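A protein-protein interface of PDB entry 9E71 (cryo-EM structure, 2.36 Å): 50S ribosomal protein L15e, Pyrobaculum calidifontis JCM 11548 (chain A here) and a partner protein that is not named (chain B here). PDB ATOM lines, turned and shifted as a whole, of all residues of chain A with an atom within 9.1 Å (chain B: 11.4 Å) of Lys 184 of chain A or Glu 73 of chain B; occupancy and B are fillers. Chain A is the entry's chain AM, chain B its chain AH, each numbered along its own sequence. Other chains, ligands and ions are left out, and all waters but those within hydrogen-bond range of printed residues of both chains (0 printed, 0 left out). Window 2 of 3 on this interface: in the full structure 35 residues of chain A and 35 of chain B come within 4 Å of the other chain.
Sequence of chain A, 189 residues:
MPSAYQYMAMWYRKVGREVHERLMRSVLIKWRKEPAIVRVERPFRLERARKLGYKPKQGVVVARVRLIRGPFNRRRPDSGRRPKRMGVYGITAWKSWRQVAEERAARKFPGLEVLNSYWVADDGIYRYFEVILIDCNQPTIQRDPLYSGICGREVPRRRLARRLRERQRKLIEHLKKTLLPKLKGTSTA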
ATOM      1  N   ILE A 172      10.230  -2.967 -30.309  1.00  0.00           N
ATOM      2  CA  ILE A 172      11.437  -3.285 -29.546  1.00  0.00           C
ATOM      3  C   ILE A 172      11.926  -4.686 -29.874  1.00  0.00           C
ATOM      4  O   ILE A 172      13.136  -4.920 -29.992  1.00  0.00           O
ATOM      5  CB  ILE A 172      11.206  -3.128 -28.033  1.00  0.00           C
ATOM      6  CG1 ILE A 172      10.564  -1.785 -27.708  1.00  0.00           C
ATOM      7  CG2 ILE A 172      12.511  -3.319 -27.280  1.00  0.00           C
ATOM      8  CD1 ILE A 172      10.837  -1.327 -26.299  1.00  0.00           C
ATOM      9  N   LEU A 175      13.593  -4.507 -33.288  1.00  0.00           N
ATOM     10  CA  LEU A 175      14.827  -3.730 -33.267  1.00  0.00           C
ATOM     11  C   LEU A 175      15.937  -4.436 -32.506  1.00  0.00           C
ATOM     12  O   LEU A 175      17.116  -4.188 -32.781  1.00  0.00           O
ATOM     13  CB  LEU A 175      14.573  -2.352 -32.660  1.00  0.00           C
ATOM     14  CG  LEU A 175      13.734  -1.386 -33.491  1.00  0.00           C
ATOM     15  CD1 LEU A 175      13.561  -0.080 -32.749  1.00  0.00           C
ATOM     16  CD2 LEU A 175      14.373  -1.156 -34.846  1.00  0.00           C
ATOM     17  N   LYS A 176      15.583  -5.306 -31.550  1.00  0.00           N
ATOM     18  CA  LYS A 176      16.581  -6.131 -30.871  1.00  0.00           C
ATOM     19  C   LYS A 176      17.349  -6.989 -31.861  1.00  0.00           C
ATOM     20  O   LYS A 176      18.562  -7.180 -31.722  1.00  0.00           O
ATOM     21  CB  LYS A 176      15.905  -7.022 -29.831  1.00  0.00           C
ATOM     22  CG  LYS A 176      15.802  -6.428 -28.446  1.00  0.00           C
ATOM     23  CD  LYS A 176      14.953  -7.317 -27.555  1.00  0.00           C
ATOM     24  CE  LYS A 176      15.206  -7.050 -26.084  1.00  0.00           C
ATOM     25  NZ  LYS A 176      16.448  -7.716 -25.607  1.00  0.00           N
ATOM     26  N   LYS A 177      16.659  -7.503 -32.877  1.00  0.00           N
ATOM     27  CA  LYS A 177      17.314  -8.297 -33.906  1.00  0.00           C
ATOM     28  C   LYS A 177      17.984  -7.417 -34.953  1.00  0.00           C
ATOM     29  O   LYS A 177      19.139  -7.649 -35.323  1.00  0.00           O
ATOM     30  CB  LYS A 177      16.297  -9.212 -34.583  1.00  0.00           C
ATOM     31  CG  LYS A 177      15.566 -10.163 -33.665  1.00  0.00           C
ATOM     32  CD  LYS A 177      14.388 -10.807 -34.384  1.00  0.00           C
ATOM     33  CE  LYS A 177      14.575 -10.816 -35.899  1.00  0.00           C
ATOM     34  NZ  LYS A 177      15.674 -11.715 -36.364  1.00  0.00           N
ATOM     35  N   LEU A 179      18.688  -4.027 -35.225  1.00  0.00           N
ATOM     36  CA  LEU A 179      19.379  -2.752 -35.079  1.00  0.00           C
ATOM     37  C   LEU A 179      20.491  -2.778 -34.046  1.00  0.00           C
ATOM     38  O   LEU A 179      21.422  -1.975 -34.142  1.00  0.00           O
ATOM     39  CB  LEU A 179      18.368  -1.651 -34.717  1.00  0.00           C
ATOM     40  CG  LEU A 179      18.955  -0.254 -34.525  1.00  0.00           C
ATOM     41  CD1 LEU A 179      19.631   0.204 -35.795  1.00  0.00           C
ATOM     42  CD2 LEU A 179      17.876   0.721 -34.110  1.00  0.00           C
ATOM     43  N   LEU A 180      20.407  -3.660 -33.055  1.00  0.00           N
ATOM     44  CA  LEU A 180      21.388  -3.691 -31.973  1.00  0.00           C
ATOM     45  C   LEU A 180      22.812  -3.980 -32.434  1.00  0.00           C
ATOM     46  O   LEU A 180      23.732  -3.289 -31.967  1.00  0.00           O
ATOM     47  CB  LEU A 180      20.934  -4.709 -30.920  1.00  0.00           C
ATOM     48  CG  LEU A 180      21.808  -4.812 -29.672  1.00  0.00           C
ATOM     49  CD1 LEU A 180      21.984  -3.444 -29.041  1.00  0.00           C
ATOM     50  CD2 LEU A 180      21.200  -5.794 -28.679  1.00  0.00           C
ATOM     51  N   PRO A 181      23.078  -4.978 -33.288  1.00  0.00           N
ATOM     52  CA  PRO A 181      24.457  -5.159 -33.781  1.00  0.00           C
ATOM     53  C   PRO A 181      24.996  -3.970 -34.560  1.00  0.00           C
ATOM     54  O   PRO A 181      26.171  -3.616 -34.399  1.00  0.00           O
ATOM     55  CB  PRO A 181      24.350  -6.409 -34.663  1.00  0.00           C
ATOM     56  CG  PRO A 181      23.183  -7.140 -34.143  1.00  0.00           C
ATOM     57  CD  PRO A 181      22.215  -6.115 -33.659  1.00  0.00           C
ATOM     58  N   LYS A 182      24.168  -3.333 -35.390  1.00  0.00           N
ATOM     59  CA  LYS A 182      24.626  -2.158 -36.123  1.00  0.00           C
ATOM     60  C   LYS A 182      24.900  -0.996 -35.178  1.00  0.00           C
ATOM     61  O   LYS A 182      25.846  -0.227 -35.382  1.00  0.00           O
ATOM     62  CB  LYS A 182      23.595  -1.761 -37.177  1.00  0.00           C
ATOM     63  CG  LYS A 182      23.162  -2.896 -38.086  1.00  0.00           C
ATOM     64  CD  LYS A 182      21.816  -2.603 -38.726  1.00  0.00           C
ATOM     65  CE  LYS A 182      21.755  -3.118 -40.154  1.00  0.00           C
ATOM     66  NZ  LYS A 182      20.472  -2.760 -40.821  1.00  0.00           N
ATOM     67  N   LEU A 183      24.072  -0.848 -34.143  1.00  0.00           N
ATOM     68  CA  LEU A 183      24.292   0.202 -33.155  1.00  0.00           C
ATOM     69  C   LEU A 183      25.587  -0.029 -32.388  1.00  0.00           C
ATOM     70  O   LEU A 183      26.370   0.902 -32.171  1.00  0.00           O
ATOM     71  CB  LEU A 183      23.107   0.259 -32.194  1.00  0.00           C
ATOM     72  CG  LEU A 183      21.800   0.788 -32.771  1.00  0.00           C
ATOM     73  CD1 LEU A 183      20.706   0.663 -31.739  1.00  0.00           C
ATOM     74  CD2 LEU A 183      21.963   2.229 -33.214  1.00  0.00           C
ATOM     75  N   LYS A 184      25.829  -1.270 -31.967  1.00  0.00           N
ATOM     76  CA  LYS A 184      26.984  -1.554 -31.124  1.00  0.00           C
ATOM     77  C   LYS A 184      28.289  -1.566 -31.909  1.00  0.00           C
ATOM     78  O   LYS A 184      29.321  -1.133 -31.386  1.00  0.00           O
ATOM     79  CB  LYS A 184      26.791  -2.889 -30.406  1.00  0.00           C
ATOM     80  CG  LYS A 184      26.353  -2.747 -28.960  1.00  0.00           C
ATOM     81  CD  LYS A 184      26.362  -4.086 -28.242  1.00  0.00           C
ATOM     82  CE  LYS A 184      25.224  -4.970 -28.719  1.00  0.00           C
ATOM     83  NZ  LYS A 184      24.557  -5.678 -27.592  1.00  0.00           N
ATOM     84  N   GLY A 185      28.270  -2.052 -33.146  1.00  0.00           N
ATOM     85  CA  GLY A 185      29.471  -2.101 -33.955  1.00  0.00           C
ATOM     86  C   GLY A 185      29.994  -0.730 -34.330  1.00  0.00           C
ATOM     87  O   GLY A 185      30.090  -0.395 -35.509  1.00  0.00           O
ATOM     88  N   GLU B  34      20.684   8.699 -38.642  1.00  0.00           N
ATOM     89  CA  GLU B  34      22.023   8.303 -38.220  1.00  0.00           C
ATOM     90  C   GLU B  34      22.020   7.049 -37.352  1.00  0.00           C
ATOM     91  O   GLU B  34      23.015   6.318 -37.338  1.00  0.00           O
ATOM     92  CB  GLU B  34      22.687   9.449 -37.462  1.00  0.00           C
ATOM     93  CG  GLU B  34      23.868  10.064 -38.173  1.00  0.00           C
ATOM     94  CD  GLU B  34      25.068   9.142 -38.208  1.00  0.00           C
ATOM     95  OE1 GLU B  34      25.749   9.010 -37.169  1.00  0.00           O
ATOM     96  OE2 GLU B  34      25.331   8.549 -39.274  1.00  0.00           O
ATOM     97  N   VAL B  35      20.935   6.783 -36.626  1.00  0.00           N
ATOM     98  CA  VAL B  35      20.841   5.619 -35.758  1.00  0.00           C
ATOM     99  C   VAL B  35      19.904   4.555 -36.306  1.00  0.00           C
ATOM    100  O   VAL B  35      19.814   3.465 -35.724  1.00  0.00           O
ATOM    101  CB  VAL B  35      20.422   6.018 -34.333  1.00  0.00           C
ATOM    102  CG1 VAL B  35      21.591   6.646 -33.604  1.00  0.00           C
ATOM    103  CG2 VAL B  35      19.249   6.971 -34.380  1.00  0.00           C
ATOM    104  N   GLY B  36      19.195   4.836 -37.395  1.00  0.00           N
ATOM    105  CA  GLY B  36      18.434   3.804 -38.069  1.00  0.00           C
ATOM    106  C   GLY B  36      16.967   3.717 -37.718  1.00  0.00           C
ATOM    107  O   GLY B  36      16.394   2.626 -37.764  1.00  0.00           O
ATOM    108  N   LEU B  45       8.974   4.350 -29.826  1.00  0.00           N
ATOM    109  CA  LEU B  45       9.899   4.192 -28.711  1.00  0.00           C
ATOM    110  C   LEU B  45       9.729   5.263 -27.645  1.00  0.00           C
ATOM    111  O   LEU B  45      10.215   5.079 -26.526  1.00  0.00           O
ATOM    112  CB  LEU B  45      11.342   4.201 -29.208  1.00  0.00           C
ATOM    113  CG  LEU B  45      11.736   3.018 -30.085  1.00  0.00           C
ATOM    114  CD1 LEU B  45      13.139   3.205 -30.621  1.00  0.00           C
ATOM    115  CD2 LEU B  45      11.611   1.715 -29.309  1.00  0.00           C
ATOM    116  N   VAL B  61      23.217  12.677 -31.557  1.00  0.00           N
ATOM    117  CA  VAL B  61      23.375  11.351 -32.154  1.00  0.00           C
ATOM    118  C   VAL B  61      23.973  10.375 -31.149  1.00  0.00           C
ATOM    119  O   VAL B  61      23.524   9.230 -31.027  1.00  0.00           O
ATOM    120  CB  VAL B  61      24.231  11.434 -33.430  1.00  0.00           C
ATOM    121  CG1 VAL B  61      24.357  10.063 -34.060  1.00  0.00           C
ATOM    122  CG2 VAL B  61      23.625  12.422 -34.410  1.00  0.00           C
ATOM    123  N   GLU B  62      24.995  10.816 -30.410  1.00  0.00           N
ATOM    124  CA  GLU B  62      25.633   9.945 -29.427  1.00  0.00           C
ATOM    125  C   GLU B  62      24.681   9.589 -28.293  1.00  0.00           C
ATOM    126  O   GLU B  62      24.634   8.431 -27.858  1.00  0.00           O
ATOM    127  CB  GLU B  62      26.899  10.602 -28.872  1.00  0.00           C
ATOM    128  CG  GLU B  62      27.906  11.035 -29.924  1.00  0.00           C
ATOM    129  CD  GLU B  62      28.110  10.000 -31.015  1.00  0.00           C
ATOM    130  OE1 GLU B  62      28.115   8.789 -30.699  1.00  0.00           O
ATOM    131  OE2 GLU B  62      28.263  10.397 -32.189  1.00  0.00           O
ATOM    132  N   LEU B  64      21.400   9.510 -28.461  1.00  0.00           N
ATOM    133  CA  LEU B  64      20.412   8.601 -29.031  1.00  0.00           C
ATOM    134  C   LEU B  64      20.960   7.186 -29.141  1.00  0.00           C
ATOM    135  O   LEU B  64      20.277   6.218 -28.789  1.00  0.00           O
ATOM    136  CB  LEU B  64      19.971   9.098 -30.403  1.00  0.00           C
ATOM    137  CG  LEU B  64      18.931  10.209 -30.446  1.00  0.00           C
ATOM    138  CD1 LEU B  64      18.767  10.684 -31.876  1.00  0.00           C
ATOM    139  CD2 LEU B  64      17.615   9.722 -29.879  1.00  0.00           C
ATOM    140  N   ARG B  65      22.199   7.051 -29.627  1.00  0.00           N
ATOM    141  CA  ARG B  65      22.799   5.730 -29.794  1.00  0.00           C
ATOM    142  C   ARG B  65      22.972   5.030 -28.457  1.00  0.00           C
ATOM    143  O   ARG B  65      22.659   3.840 -28.328  1.00  0.00           O
ATOM    144  CB  ARG B  65      24.145   5.845 -30.505  1.00  0.00           C
ATOM    145  CG  ARG B  65      24.810   4.509 -30.773  1.00  0.00           C
ATOM    146  CD  ARG B  65      25.267   4.388 -32.216  1.00  0.00           C
ATOM    147  NE  ARG B  65      26.231   5.423 -32.570  1.00  0.00           N
ATOM    148  CZ  ARG B  65      26.299   6.016 -33.755  1.00  0.00           C
ATOM    149  NH1 ARG B  65      25.454   5.716 -34.728  1.00  0.00           N
ATOM    150  NH2 ARG B  65      27.239   6.930 -33.968  1.00  0.00           N
ATOM    151  N   LYS B  66      23.434   5.767 -27.441  1.00  0.00           N
ATOM    152  CA  LYS B  66      23.621   5.181 -26.118  1.00  0.00           C
ATOM    153  C   LYS B  66      22.300   4.700 -25.534  1.00  0.00           C
ATOM    154  O   LYS B  66      22.171   3.530 -25.145  1.00  0.00           O
ATOM    155  CB  LYS B  66      24.280   6.196 -25.188  1.00  0.00           C
ATOM    156  CG  LYS B  66      24.380   5.726 -23.755  1.00  0.00           C
ATOM    157  CD  LYS B  66      25.463   6.469 -23.002  1.00  0.00           C
ATOM    158  CE  LYS B  66      25.400   6.159 -21.519  1.00  0.00           C
ATOM    159  NZ  LYS B  66      24.213   6.786 -20.882  1.00  0.00           N
ATOM    160  N   TRP B  67      21.289   5.577 -25.513  1.00  0.00           N
ATOM    161  CA  TRP B  67      20.012   5.206 -24.912  1.00  0.00           C
ATOM    162  C   TRP B  67      19.328   4.087 -25.685  1.00  0.00           C
ATOM    163  O   TRP B  67      18.699   3.208 -25.087  1.00  0.00           O
ATOM    164  CB  TRP B  67      19.094   6.416 -24.824  1.00  0.00           C
ATOM    165  CG  TRP B  67      17.824   6.117 -24.115  1.00  0.00           C
ATOM    166  CD1 TRP B  67      17.623   6.103 -22.770  1.00  0.00           C
ATOM    167  CD2 TRP B  67      16.570   5.780 -24.712  1.00  0.00           C
ATOM    168  NE1 TRP B  67      16.318   5.784 -22.489  1.00  0.00           N
ATOM    169  CE2 TRP B  67      15.651   5.579 -23.667  1.00  0.00           C
ATOM    170  CE3 TRP B  67      16.135   5.630 -26.031  1.00  0.00           C
ATOM    171  CZ2 TRP B  67      14.323   5.240 -23.898  1.00  0.00           C
ATOM    172  CZ3 TRP B  67      14.819   5.290 -26.259  1.00  0.00           C
ATOM    173  CH2 TRP B  67      13.928   5.098 -25.198  1.00  0.00           C
ATOM    174  N   LEU B  68      19.450   4.091 -27.013  1.00  0.00           N
ATOM    175  CA  LEU B  68      18.853   3.020 -27.794  1.00  0.00           C
ATOM    176  C   LEU B  68      19.569   1.703 -27.543  1.00  0.00           C
ATOM    177  O   LEU B  68      18.946   0.637 -27.585  1.00  0.00           O
ATOM    178  CB  LEU B  68      18.870   3.384 -29.276  1.00  0.00           C
ATOM    179  CG  LEU B  68      18.285   2.355 -30.241  1.00  0.00           C
ATOM    180  CD1 LEU B  68      16.970   1.816 -29.714  1.00  0.00           C
ATOM    181  CD2 LEU B  68      18.096   2.976 -31.615  1.00  0.00           C
ATOM    182  N   ILE B  69      20.874   1.754 -27.258  1.00  0.00           N
ATOM    183  CA  ILE B  69      21.598   0.532 -26.918  1.00  0.00           C
ATOM    184  C   ILE B  69      21.108  -0.028 -25.588  1.00  0.00           C
ATOM    185  O   ILE B  69      20.898  -1.239 -25.454  1.00  0.00           O
ATOM    186  CB  ILE B  69      23.114   0.786 -26.902  1.00  0.00           C
ATOM    187  CG1 ILE B  69      23.688   0.581 -28.302  1.00  0.00           C
ATOM    188  CG2 ILE B  69      23.789  -0.153 -25.931  1.00  0.00           C
ATOM    189  CD1 ILE B  69      25.186   0.706 -28.374  1.00  0.00           C
ATOM    190  N   GLU B  70      20.918   0.843 -24.584  1.00  0.00           N
ATOM    191  CA  GLU B  70      20.329   0.368 -23.326  1.00  0.00           C
ATOM    192  C   GLU B  70      18.927  -0.199 -23.532  1.00  0.00           C
ATOM    193  O   GLU B  70      18.566  -1.214 -22.927  1.00  0.00           O
ATOM    194  CB  GLU B  70      20.271   1.453 -22.242  1.00  0.00           C
ATOM    195  CG  GLU B  70      21.469   1.508 -21.286  1.00  0.00           C
ATOM    196  CD  GLU B  70      22.478   2.594 -21.564  1.00  0.00           C
ATOM    197  OE1 GLU B  70      22.299   3.345 -22.524  1.00  0.00           O
ATOM    198  OE2 GLU B  70      23.462   2.705 -20.807  1.00  0.00           O
ATOM    199  N   VAL B  71      18.122   0.451 -24.375  1.00  0.00           N
ATOM    200  CA  VAL B  71      16.752  -0.004 -24.594  1.00  0.00           C
ATOM    201  C   VAL B  71      16.735  -1.368 -25.266  1.00  0.00           C
ATOM    202  O   VAL B  71      15.982  -2.263 -24.869  1.00  0.00           O
ATOM    203  CB  VAL B  71      15.974   1.035 -25.418  1.00  0.00           C
ATOM    204  CG1 VAL B  71      14.653   0.448 -25.887  1.00  0.00           C
ATOM    205  CG2 VAL B  71      15.758   2.291 -24.603  1.00  0.00           C
ATOM    206  N   LEU B  72      17.563  -1.551 -26.295  1.00  0.00           N
ATOM    207  CA  LEU B  72      17.602  -2.825 -26.994  1.00  0.00           C
ATOM    208  C   LEU B  72      18.232  -3.926 -26.154  1.00  0.00           C
ATOM    209  O   LEU B  72      17.856  -5.092 -26.306  1.00  0.00           O
ATOM    210  CB  LEU B  72      18.350  -2.670 -28.314  1.00  0.00           C
ATOM    211  CG  LEU B  72      17.639  -1.706 -29.258  1.00  0.00           C
ATOM    212  CD1 LEU B  72      18.378  -1.591 -30.575  1.00  0.00           C
ATOM    213  CD2 LEU B  72      16.205  -2.157 -29.473  1.00  0.00           C
ATOM    214  N   GLU B  73      19.163  -3.587 -25.266  1.00  0.00           N
ATOM    215  CA  GLU B  73      19.730  -4.560 -24.347  1.00  0.00           C
ATOM    216  C   GLU B  73      18.896  -4.727 -23.088  1.00  0.00           C
ATOM    217  O   GLU B  73      19.300  -5.467 -22.189  1.00  0.00           O
ATOM    218  CB  GLU B  73      21.160  -4.166 -23.978  1.00  0.00           C
ATOM    219  CG  GLU B  73      22.076  -4.046 -25.183  1.00  0.00           C
ATOM    220  CD  GLU B  73      23.509  -3.737 -24.806  1.00  0.00           C
ATOM    221  OE1 GLU B  73      23.721  -3.012 -23.813  1.00  0.00           O
ATOM    222  OE2 GLU B  73      24.425  -4.216 -25.508  1.00  0.00           O
ATOM    223  N   GLY B  74      17.765  -4.038 -22.989  1.00  0.00           N
ATOM    224  CA  GLY B  74      16.820  -4.317 -21.929  1.00  0.00           C
ATOM    225  C   GLY B  74      17.178  -3.740 -20.582  1.00  0.00           C
ATOM    226  O   GLY B  74      16.500  -4.049 -19.596  1.00  0.00           O
ATOM    227  N   LYS B  75      18.218  -2.916 -20.506  1.00  0.00           N
ATOM    228  CA  LYS B  75      18.583  -2.255 -19.263  1.00  0.00           C
ATOM    229  C   LYS B  75      17.826  -0.957 -19.038  1.00  0.00           C
ATOM    230  O   LYS B  75      18.065  -0.286 -18.029  1.00  0.00           O
ATOM    231  CB  LYS B  75      20.091  -1.993 -19.232  1.00  0.00           C
ATOM    232  CG  LYS B  75      20.919  -3.129 -19.808  1.00  0.00           C
ATOM    233  CD  LYS B  75      22.409  -2.852 -19.701  1.00  0.00           C
ATOM    234  CE  LYS B  75      22.760  -1.443 -20.150  1.00  0.00           C
ATOM    235  NZ  LYS B  75      22.783  -1.333 -21.637  1.00  0.00           N
ATOM    236  N   ALA B  76      16.923  -0.587 -19.944  1.00  0.00           N
ATOM    237  CA  ALA B  76      16.121   0.614 -19.789  1.00  0.00           C
ATOM    238  C   ALA B  76      14.718   0.365 -20.321  1.00  0.00           C
ATOM    239  O   ALA B  76      14.538  -0.340 -21.317  1.00  0.00           O
ATOM    240  CB  ALA B  76      16.751   1.808 -20.517  1.00  0.00           C
ATOM    241  N   THR B  77      13.729   0.951 -19.646  1.00  0.00           N
ATOM    242  CA  THR B  77      12.343   0.871 -20.078  1.00  0.00           C
ATOM    243  C   THR B  77      11.985   2.128 -20.854  1.00  0.00           C
ATOM    244  O   THR B  77      12.067   3.231 -20.292  1.00  0.00           O
ATOM    245  CB  THR B  77      11.415   0.714 -18.882  1.00  0.00           C
ATOM    246  OG1 THR B  77      12.012  -0.168 -17.925  1.00  0.00           O
ATOM    247  CG2 THR B  77      10.079   0.143 -19.323  1.00  0.00           C
ATOM    248  N   PRO B  78      11.596   2.026 -22.126  1.00  0.00           N
ATOM    249  CA  PRO B  78      11.197   3.222 -22.855  1.00  0.00           C
ATOM    250  C   PRO B  78       9.885   3.756 -22.326  1.00  0.00           C
ATOM    251  O   PRO B  78       9.063   2.999 -21.778  1.00  0.00           O
ATOM    252  CB  PRO B  78      11.060   2.722 -24.305  1.00  0.00           C
ATOM    253  CG  PRO B  78      10.733   1.283 -24.171  1.00  0.00           C
ATOM    254  CD  PRO B  78      11.338   0.791 -22.884  1.00  0.00           C
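Leu 45 of chain B touches Ile 172 of chain A (CD2 to CG1, 3.99 Å). CG of Pro 78 of chain B touches CD1 of Ile 172 of chain A (3.4 Å). Leu 45 of chain B touches Leu 175 of chain A (CD1 to CD1, 3.9 Å). CD1 of Leu 179 of chain A touches O of Val 35 of chain B (3.3 Å). Leu 72 of chain B touches Leu 180 of chain A. Leu 180 of chain A touches Glu 73 of chain B. O of Leu 183 of chain A touches CD of Arg 65 of chain B, at 3.7 Å. Leu 68 of chain B touches Leu 183 of chain A. Leu 183 of chain A touches Ile 69 of chain B (CB to CG1, 3.9 Å). Lys 184 of chain A touches Ile 69 of chain B (CG to CD1, 3.7 Å).
Of the 11 printed residues of chain A, 7 touch a printed residue of chain B. Printed residues of chain A that touch a printed residue of chain B: Ile 172, Leu 175, Lys 176, Leu 179, Leu 180, Leu 183 and Lys 184. Printed residues of chain B that touch a printed residue of chain A: Val 35, Leu 45, Arg 65, Leu 68, Ile 69, Leu 72, Glu 73 and Pro 78. Hydrophobic or aromatic side chains of chain B within 4 Å of the printed part of chain A: Leu 45, Leu 68, Ile 69, Leu 72 and Pro 78. Among the printed residues, 16 pairs touch across the chains. Among the printed residues, Asp or Glu carboxylates within 4 Å of a Lys or Arg side-chain nitrogen of the other chain: Lys 184 of chain A with Glu 73 of chain B (2.5 Å).
The backbone NH of Leu 180 of chain A lies within hydrogen-bond range of the backbone carbonyl oxygen of Leu 175 of chain A (3.3 Å). The side-chain carboxylate of Glu 62 of chain B lies within salt-bridge range of the guanidinium group of Arg 65 of chain B, at 3.9 Å. The side-chain carboxylate (OE1) of Glu 73 of chain B is in salt-bridge range of the side-chain amino group (NZ) of Lys 75 of chain B (2.9 Å).
NZ of Lys 176 of chain A sits at hydrogen-bond distance from O of Leu 72 of chain B (3.1 Å). The side-chain amino group of Lys 184 of chain A is in salt-bridge range of the side-chain carboxylate of Glu 73 of chain B (2.5 Å).
Printed residues of chain B within 4 Å of Ile 172 of chain A: Leu 45 (3.99 Å) and Pro 78 (3.4 Å). Of the printed residues of chain B, Lys 176 of chain A touches Leu 72. Printed residues of chain B within 4 Å of Leu 179 of chain A: Val 35 (3.3 Å) and Leu 68 (3.4 Å). Of chain B, only Leu 72 and Glu 73 come within 4 Å of Leu 180 of chain A. No residue of chain B comes within 4 Å of Pro 181 of chain A. Lys 182 of chain A touches none of the printed residues of chain B. Lys 184 of chain A touches just these residues of chain B: Ile 69 (3.7 Å) and Glu 73 (2.5 Å). No residue of chain B comes within 4 Å of Gly 185 of chain A. Of the printed residues of chain A, Ile 69 of chain B touches Leu 183 and Lys 184. Val 71 of chain B touches none of the printed residues of chain A. Glu 73 of chain B touches two residues of chain A. The nearest residue of chain B that does not touch Lys 184 of chain A is Arg 65 of chain B (5.7 Å).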
